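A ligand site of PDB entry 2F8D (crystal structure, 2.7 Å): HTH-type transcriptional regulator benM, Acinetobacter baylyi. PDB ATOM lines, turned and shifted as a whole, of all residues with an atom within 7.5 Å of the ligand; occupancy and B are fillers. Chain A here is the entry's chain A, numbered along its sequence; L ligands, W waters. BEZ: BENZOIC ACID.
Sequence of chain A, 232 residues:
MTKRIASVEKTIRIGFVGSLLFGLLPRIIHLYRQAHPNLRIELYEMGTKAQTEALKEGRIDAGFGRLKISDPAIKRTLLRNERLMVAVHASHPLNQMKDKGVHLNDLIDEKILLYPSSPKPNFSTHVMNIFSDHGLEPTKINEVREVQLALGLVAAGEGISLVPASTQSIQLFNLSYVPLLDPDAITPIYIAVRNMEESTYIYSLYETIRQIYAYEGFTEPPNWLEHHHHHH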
ATOM      1  N   VAL A  17     -10.288 -11.852 -32.255  1.00  0.00           N
ATOM      2  CA  VAL A  17      -8.967 -12.072 -31.659  1.00  0.00           C
ATOM      3  C   VAL A  17      -8.761 -13.575 -31.554  1.00  0.00           C
ATOM      4  O   VAL A  17      -9.649 -14.309 -31.117  1.00  0.00           O
ATOM      5  CB  VAL A  17      -8.894 -11.365 -30.284  1.00  0.00           C
ATOM      6  CG1 VAL A  17      -7.853 -11.970 -29.395  1.00  0.00           C
ATOM      7  CG2 VAL A  17      -8.639  -9.885 -30.468  1.00  0.00           C
ATOM      8  N   GLY A  18      -7.579 -14.049 -31.974  1.00  0.00           N
ATOM      9  CA  GLY A  18      -7.284 -15.487 -32.086  1.00  0.00           C
ATOM     10  C   GLY A  18      -7.711 -16.383 -30.927  1.00  0.00           C
ATOM     11  O   GLY A  18      -8.350 -17.418 -31.143  1.00  0.00           O
ATOM     12  N   SER A  19      -7.366 -15.965 -29.709  1.00  0.00           N
ATOM     13  CA  SER A  19      -7.624 -16.763 -28.503  1.00  0.00           C
ATOM     14  C   SER A  19      -9.093 -17.131 -28.303  1.00  0.00           C
ATOM     15  O   SER A  19      -9.412 -18.180 -27.720  1.00  0.00           O
ATOM     16  CB  SER A  19      -7.084 -16.053 -27.248  1.00  0.00           C
ATOM     17  OG  SER A  19      -7.809 -14.863 -26.985  1.00  0.00           O
ATOM     18  N   LEU A  20     -10.000 -16.295 -28.801  1.00  0.00           N
ATOM     19  CA  LEU A  20     -11.419 -16.568 -28.685  1.00  0.00           C
ATOM     20  C   LEU A  20     -11.865 -17.849 -29.435  1.00  0.00           C
ATOM     21  O   LEU A  20     -12.935 -18.392 -29.155  1.00  0.00           O
ATOM     22  CB  LEU A  20     -12.254 -15.354 -29.103  1.00  0.00           C
ATOM     23  CG  LEU A  20     -12.009 -14.062 -28.320  1.00  0.00           C
ATOM     24  CD1 LEU A  20     -12.880 -12.937 -28.830  1.00  0.00           C
ATOM     25  CD2 LEU A  20     -12.192 -14.244 -26.813  1.00  0.00           C
ATOM     26  N   GLU A  45      -9.254 -12.443 -38.543  1.00  0.00           N
ATOM     27  CA  GLU A  45      -8.450 -12.273 -37.357  1.00  0.00           C
ATOM     28  C   GLU A  45      -7.857 -10.862 -37.373  1.00  0.00           C
ATOM     29  O   GLU A  45      -7.165 -10.485 -38.324  1.00  0.00           O
ATOM     30  CB  GLU A  45      -7.330 -13.291 -37.292  1.00  0.00           C
ATOM     31  CG  GLU A  45      -6.754 -13.364 -35.903  1.00  0.00           C
ATOM     32  CD  GLU A  45      -5.385 -13.985 -35.831  1.00  0.00           C
ATOM     33  OE1 GLU A  45      -4.802 -14.341 -36.880  1.00  0.00           O
ATOM     34  OE2 GLU A  45      -4.876 -14.108 -34.698  1.00  0.00           O
ATOM     35  N   GLY A  47      -6.682  -7.436 -34.352  1.00  0.00           N
ATOM     36  CA  GLY A  47      -6.617  -6.849 -33.017  1.00  0.00           C
ATOM     37  C   GLY A  47      -7.659  -5.770 -32.812  1.00  0.00           C
ATOM     38  O   GLY A  47      -8.356  -5.375 -33.756  1.00  0.00           O
ATOM     39  N   THR A  48      -7.757  -5.276 -31.577  1.00  0.00           N
ATOM     40  CA  THR A  48      -8.764  -4.301 -31.178  1.00  0.00           C
ATOM     41  C   THR A  48      -8.622  -2.982 -31.948  1.00  0.00           C
ATOM     42  O   THR A  48      -9.616  -2.374 -32.366  1.00  0.00           O
ATOM     43  CB  THR A  48      -8.717  -4.104 -29.625  1.00  0.00           C
ATOM     44  OG1 THR A  48      -9.246  -5.272 -28.982  1.00  0.00           O
ATOM     45  CG2 THR A  48      -9.540  -2.897 -29.184  1.00  0.00           C
ATOM     46  N   GLY A  65     -13.206  -9.038 -29.065  1.00  0.00           N
ATOM     47  CA  GLY A  65     -11.899  -8.685 -28.582  1.00  0.00           C
ATOM     48  C   GLY A  65     -11.802  -8.699 -27.085  1.00  0.00           C
ATOM     49  O   GLY A  65     -12.779  -8.947 -26.387  1.00  0.00           O
ATOM     50  N   ARG A  66     -10.607  -8.393 -26.609  1.00  0.00           N
ATOM     51  CA  ARG A  66     -10.238  -8.585 -25.222  1.00  0.00           C
ATOM     52  C   ARG A  66      -9.778  -7.281 -24.562  1.00  0.00           C
ATOM     53  O   ARG A  66      -9.569  -7.240 -23.352  1.00  0.00           O
ATOM     54  CB  ARG A  66      -9.101  -9.592 -25.167  1.00  0.00           C
ATOM     55  CG  ARG A  66      -9.451 -10.996 -25.664  1.00  0.00           C
ATOM     56  CD  ARG A  66      -9.820 -11.853 -24.506  1.00  0.00           C
ATOM     57  NE  ARG A  66      -9.527 -13.256 -24.760  1.00  0.00           N
ATOM     58  CZ  ARG A  66      -9.951 -14.257 -24.005  1.00  0.00           C
ATOM     59  NH1 ARG A  66     -10.697 -14.034 -22.921  1.00  0.00           N
ATOM     60  NH2 ARG A  66      -9.636 -15.494 -24.334  1.00  0.00           N
ATOM     61  N   LEU A  67      -9.627  -6.235 -25.375  1.00  0.00           N
ATOM     62  CA  LEU A  67      -9.249  -4.915 -24.891  1.00  0.00           C
ATOM     63  C   LEU A  67     -10.410  -3.925 -24.964  1.00  0.00           C
ATOM     64  O   LEU A  67     -11.339  -4.107 -25.743  1.00  0.00           O
ATOM     65  CB  LEU A  67      -8.052  -4.376 -25.688  1.00  0.00           C
ATOM     66  CG  LEU A  67      -6.694  -5.046 -25.449  1.00  0.00           C
ATOM     67  CD1 LEU A  67      -5.667  -4.570 -26.473  1.00  0.00           C
ATOM     68  CD2 LEU A  67      -6.167  -4.821 -24.036  1.00  0.00           C
ATOM     69  N   LYS A  68     -10.346  -2.877 -24.144  1.00  0.00           N
ATOM     70  CA  LYS A  68     -11.369  -1.832 -24.149  1.00  0.00           C
ATOM     71  C   LYS A  68     -11.065  -0.818 -25.250  1.00  0.00           C
ATOM     72  O   LYS A  68      -9.902  -0.519 -25.524  1.00  0.00           O
ATOM     73  CB  LYS A  68     -11.436  -1.141 -22.794  1.00  0.00           C
ATOM     74  CG  LYS A  68     -11.473  -2.090 -21.608  1.00  0.00           C
ATOM     75  CD  LYS A  68     -11.904  -1.378 -20.349  1.00  0.00           C
ATOM     76  CE  LYS A  68     -11.173  -1.907 -19.120  1.00  0.00           C
ATOM     77  NZ  LYS A  68     -11.586  -3.269 -18.702  1.00  0.00           N
ATOM     78  N   GLU A  82     -13.544 -14.081 -18.519  1.00  0.00           N
ATOM     79  CA  GLU A  82     -12.985 -15.415 -18.499  1.00  0.00           C
ATOM     80  C   GLU A  82     -11.900 -15.522 -17.433  1.00  0.00           C
ATOM     81  O   GLU A  82     -11.029 -14.662 -17.320  1.00  0.00           O
ATOM     82  CB  GLU A  82     -12.417 -15.786 -19.873  1.00  0.00           C
ATOM     83  CG  GLU A  82     -11.945 -17.210 -19.945  1.00  0.00           C
ATOM     84  CD  GLU A  82     -11.613 -17.653 -21.369  1.00  0.00           C
ATOM     85  OE1 GLU A  82     -11.251 -16.794 -22.214  1.00  0.00           O
ATOM     86  OE2 GLU A  82     -11.706 -18.873 -21.614  1.00  0.00           O
ATOM     87  N   TYR A 115       2.978 -14.424 -23.814  1.00  0.00           N
ATOM     88  CA  TYR A 115       2.729 -14.558 -25.246  1.00  0.00           C
ATOM     89  C   TYR A 115       1.549 -13.692 -25.623  1.00  0.00           C
ATOM     90  O   TYR A 115       0.776 -13.303 -24.750  1.00  0.00           O
ATOM     91  CB  TYR A 115       2.460 -16.031 -25.594  1.00  0.00           C
ATOM     92  CG  TYR A 115       1.154 -16.555 -25.026  1.00  0.00           C
ATOM     93  CD1 TYR A 115      -0.027 -16.485 -25.782  1.00  0.00           C
ATOM     94  CD2 TYR A 115       1.098 -17.093 -23.738  1.00  0.00           C
ATOM     95  CE1 TYR A 115      -1.230 -16.954 -25.271  1.00  0.00           C
ATOM     96  CE2 TYR A 115      -0.119 -17.567 -23.208  1.00  0.00           C
ATOM     97  CZ  TYR A 115      -1.267 -17.489 -23.989  1.00  0.00           C
ATOM     98  OH  TYR A 115      -2.476 -17.946 -23.496  1.00  0.00           O
ATOM     99  N   PRO A 116       1.389 -13.375 -26.917  1.00  0.00           N
ATOM    100  CA  PRO A 116       2.315 -13.636 -28.012  1.00  0.00           C
ATOM    101  C   PRO A 116       3.320 -12.498 -28.202  1.00  0.00           C
ATOM    102  O   PRO A 116       3.321 -11.538 -27.420  1.00  0.00           O
ATOM    103  CB  PRO A 116       1.379 -13.732 -29.231  1.00  0.00           C
ATOM    104  CG  PRO A 116       0.206 -12.864 -28.874  1.00  0.00           C
ATOM    105  CD  PRO A 116       0.156 -12.708 -27.384  1.00  0.00           C
ATOM    106  N   SER A 118       3.376 -10.679 -30.966  1.00  0.00           N
ATOM    107  CA  SER A 118       2.713  -9.709 -31.841  1.00  0.00           C
ATOM    108  C   SER A 118       2.787  -8.270 -31.274  1.00  0.00           C
ATOM    109  O   SER A 118       3.160  -8.089 -30.128  1.00  0.00           O
ATOM    110  CB  SER A 118       1.258 -10.134 -32.030  1.00  0.00           C
ATOM    111  OG  SER A 118       0.550 -10.064 -30.796  1.00  0.00           O
ATOM    112  N   PRO A 121      -0.494  -3.108 -27.241  1.00  0.00           N
ATOM    113  CA  PRO A 121      -0.829  -4.048 -26.181  1.00  0.00           C
ATOM    114  C   PRO A 121      -1.388  -5.366 -26.715  1.00  0.00           C
ATOM    115  O   PRO A 121      -1.985  -5.410 -27.784  1.00  0.00           O
ATOM    116  CB  PRO A 121      -1.912  -3.308 -25.374  1.00  0.00           C
ATOM    117  CG  PRO A 121      -1.706  -1.908 -25.690  1.00  0.00           C
ATOM    118  CD  PRO A 121      -1.297  -1.885 -27.129  1.00  0.00           C
ATOM    119  N   ASN A 122      -1.176  -6.424 -25.956  1.00  0.00           N
ATOM    120  CA  ASN A 122      -1.723  -7.745 -26.297  1.00  0.00           C
ATOM    121  C   ASN A 122      -1.855  -8.533 -25.014  1.00  0.00           C
ATOM    122  O   ASN A 122      -1.836  -7.942 -23.914  1.00  0.00           O
ATOM    123  CB  ASN A 122      -0.831  -8.475 -27.301  1.00  0.00           C
ATOM    124  CG  ASN A 122       0.614  -8.581 -26.852  1.00  0.00           C
ATOM    125  OD1 ASN A 122       0.937  -8.480 -25.656  1.00  0.00           O
ATOM    126  ND2 ASN A 122       1.518  -8.782 -27.813  1.00  0.00           N
ATOM    127  N   PHE A 123      -1.983  -9.853 -25.128  1.00  0.00           N
ATOM    128  CA  PHE A 123      -2.173 -10.702 -23.963  1.00  0.00           C
ATOM    129  C   PHE A 123      -0.969 -10.660 -23.005  1.00  0.00           C
ATOM    130  O   PHE A 123      -1.132 -10.847 -21.801  1.00  0.00           O
ATOM    131  CB  PHE A 123      -2.513 -12.144 -24.365  1.00  0.00           C
ATOM    132  CG  PHE A 123      -2.793 -13.061 -23.210  1.00  0.00           C
ATOM    133  CD1 PHE A 123      -3.890 -12.826 -22.364  1.00  0.00           C
ATOM    134  CD2 PHE A 123      -1.984 -14.157 -22.947  1.00  0.00           C
ATOM    135  CE1 PHE A 123      -4.155 -13.674 -21.281  1.00  0.00           C
ATOM    136  CE2 PHE A 123      -2.237 -15.012 -21.862  1.00  0.00           C
ATOM    137  CZ  PHE A 123      -3.331 -14.765 -21.037  1.00  0.00           C
ATOM    138  N   SER A 124       0.223 -10.407 -23.532  1.00  0.00           N
ATOM    139  CA  SER A 124       1.398 -10.330 -22.664  1.00  0.00           C
ATOM    140  C   SER A 124       1.334  -9.052 -21.796  1.00  0.00           C
ATOM    141  O   SER A 124       1.664  -9.090 -20.596  1.00  0.00           O
ATOM    142  CB  SER A 124       2.709 -10.453 -23.444  1.00  0.00           C
ATOM    143  OG  SER A 124       3.263  -9.187 -23.769  1.00  0.00           O
ATOM    144  N   THR A 125       0.881  -7.938 -22.385  1.00  0.00           N
ATOM    145  CA  THR A 125       0.700  -6.742 -21.561  1.00  0.00           C
ATOM    146  C   THR A 125      -0.477  -6.910 -20.609  1.00  0.00           C
ATOM    147  O   THR A 125      -0.473  -6.322 -19.528  1.00  0.00           O
ATOM    148  CB  THR A 125       0.589  -5.439 -22.378  1.00  0.00           C
ATOM    149  OG1 THR A 125      -0.568  -5.488 -23.207  1.00  0.00           O
ATOM    150  CG2 THR A 125       1.826  -5.244 -23.251  1.00  0.00           C
ATOM    151  N   HIS A 126      -1.460  -7.718 -20.986  1.00  0.00           N
ATOM    152  CA  HIS A 126      -2.608  -7.959 -20.113  1.00  0.00           C
ATOM    153  C   HIS A 126      -2.198  -8.669 -18.834  1.00  0.00           C
ATOM    154  O   HIS A 126      -2.574  -8.259 -17.730  1.00  0.00           O
ATOM    155  CB  HIS A 126      -3.694  -8.764 -20.820  1.00  0.00           C
ATOM    156  CG  HIS A 126      -4.862  -9.075 -19.935  1.00  0.00           C
ATOM    157  ND1 HIS A 126      -5.775  -8.128 -19.549  1.00  0.00           N
ATOM    158  CD2 HIS A 126      -5.236 -10.233 -19.329  1.00  0.00           C
ATOM    159  CE1 HIS A 126      -6.681  -8.672 -18.760  1.00  0.00           C
ATOM    160  NE2 HIS A 126      -6.372  -9.949 -18.604  1.00  0.00           N
ATOM    161  N   VAL A 127      -1.430  -9.748 -19.009  1.00  0.00           N
ATOM    162  CA  VAL A 127      -0.933 -10.534 -17.904  1.00  0.00           C
ATOM    163  C   VAL A 127      -0.090  -9.669 -16.956  1.00  0.00           C
ATOM    164  O   VAL A 127      -0.301  -9.700 -15.746  1.00  0.00           O
ATOM    165  CB  VAL A 127      -0.166 -11.786 -18.413  1.00  0.00           C
ATOM    166  CG1 VAL A 127       0.635 -12.453 -17.291  1.00  0.00           C
ATOM    167  CG2 VAL A 127      -1.156 -12.768 -19.002  1.00  0.00           C
ATOM    168  N   PRO A 164      -5.922 -17.999 -20.524  1.00  0.00           N
ATOM    169  CA  PRO A 164      -7.367 -18.025 -20.321  1.00  0.00           C
ATOM    170  C   PRO A 164      -7.835 -19.474 -20.064  1.00  0.00           C
ATOM    171  O   PRO A 164      -7.189 -20.418 -20.541  1.00  0.00           O
ATOM    172  CB  PRO A 164      -7.936 -17.527 -21.659  1.00  0.00           C
ATOM    173  CG  PRO A 164      -6.788 -16.889 -22.365  1.00  0.00           C
ATOM    174  CD  PRO A 164      -5.552 -17.518 -21.875  1.00  0.00           C
ATOM    175  N   ILE A 186      -8.675 -12.226 -14.277  1.00  0.00           N
ATOM    176  CA  ILE A 186      -9.637 -12.469 -15.348  1.00  0.00           C
ATOM    177  C   ILE A 186      -9.143 -11.914 -16.675  1.00  0.00           C
ATOM    178  O   ILE A 186      -8.273 -11.047 -16.712  1.00  0.00           O
ATOM    179  CB  ILE A 186     -11.017 -11.802 -15.073  1.00  0.00           C
ATOM    180  CG1 ILE A 186     -10.846 -10.309 -14.766  1.00  0.00           C
ATOM    181  CG2 ILE A 186     -11.748 -12.521 -13.954  1.00  0.00           C
ATOM    182  CD1 ILE A 186     -11.753  -9.419 -15.540  1.00  0.00           C
ATOM    183  N   THR A 187      -9.722 -12.413 -17.756  1.00  0.00           N
ATOM    184  CA  THR A 187      -9.518 -11.782 -19.037  1.00  0.00           C
ATOM    185  C   THR A 187     -10.861 -11.578 -19.751  1.00  0.00           C
ATOM    186  O   THR A 187     -11.555 -12.555 -20.066  1.00  0.00           O
ATOM    187  CB  THR A 187      -8.474 -12.510 -19.905  1.00  0.00           C
ATOM    188  OG1 THR A 187      -8.511 -11.988 -21.235  1.00  0.00           O
ATOM    189  CG2 THR A 187      -8.732 -14.017 -19.931  1.00  0.00           C
ATOM    190  N   PRO A 188     -11.231 -10.314 -19.982  1.00  0.00           N
ATOM    191  CA  PRO A 188     -12.569  -9.948 -20.463  1.00  0.00           C
ATOM    192  C   PRO A 188     -12.769 -10.312 -21.925  1.00  0.00           C
ATOM    193  O   PRO A 188     -11.789 -10.393 -22.677  1.00  0.00           O
ATOM    194  CB  PRO A 188     -12.615  -8.426 -20.287  1.00  0.00           C
ATOM    195  CG  PRO A 188     -11.349  -8.053 -19.568  1.00  0.00           C
ATOM    196  CD  PRO A 188     -10.364  -9.130 -19.824  1.00  0.00           C
HETATM  197  C   BEZ L   1      -5.759 -12.020 -26.459  1.00  0.00           C
HETATM  198  O1  BEZ L   1      -6.363 -13.167 -25.887  1.00  0.00           O
HETATM  199  O2  BEZ L   1      -5.283 -12.054 -27.682  1.00  0.00           O
HETATM  200  C1  BEZ L   1      -5.669 -10.750 -25.679  1.00  0.00           C
HETATM  201  C2  BEZ L   1      -5.968 -10.755 -24.323  1.00  0.00           C
HETATM  202  C3  BEZ L   1      -5.883  -9.566 -23.597  1.00  0.00           C
HETATM  203  C4  BEZ L   1      -5.492  -8.390 -24.242  1.00  0.00           C
HETATM  204  C5  BEZ L   1      -5.204  -8.391 -25.603  1.00  0.00           C
HETATM  205  C6  BEZ L   1      -5.291  -9.572 -26.334  1.00  0.00           C
HETATM  206  O   HOH W   1      -4.784 -14.907 -24.751  1.00  0.00           O
HETATM  207  O   HOH W   2      -2.651 -11.155 -27.761  1.00  0.00           O
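Water W2 bridges an oxygen (O2) of the ligand and the backbone NH (N) of Phe 123.
An oxygen (O1) of the ligand sits at hydrogen-bond distance from the side-chain hydroxyl of Ser 19 (2.5 Å).
NE of Arg 66 is in salt-bridge range of O1 of the ligand, at 3.4 Å.
OG of Ser 19 sits at hydrogen-bond distance from NE of Arg 66.
NH1 of Arg 66 lies within hydrogen-bond range of O of Thr 187, at 3.3 Å.
The guanidinium group of Arg 66 lies within salt-bridge range of the side-chain carboxylate of Glu 82 (2.9 Å).
ND2 of Asn 122 sits at hydrogen-bond distance from O of Pro 116 (3.3 Å).
The backbone carbonyl oxygen (O) of Asn 122 is in hydrogen-bond range of the side-chain hydroxyl (OG1) of Thr 125 (2.9 Å).
The side-chain amide oxygen of Asn 122 is in hydrogen-bond range of the backbone NH of Ser 124, 3.0 Å away.
The side-chain amide nitrogen of Asn 122 is in hydrogen-bond range of the backbone carbonyl oxygen of Ser 118, 2.9 Å away.
NE2 of His 126 is in hydrogen-bond range of O of Ile 186.
Residues that only touch the ligand: Val 17, Leu 67, Asn 122, Phe 123 and His 126.
Hydrophobic or aromatic side chains within 4 Å of the ligand: Val 17, Leu 67, Phe 123 and His 126.
Seven residues have an atom within 4 Å of the ligand: Val 17, Ser 19, Arg 66, Leu 67, Asn 122, Phe 123 and His 126.
Along chain A the residues within 4 Å of the ligand span positions 17 to 126.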
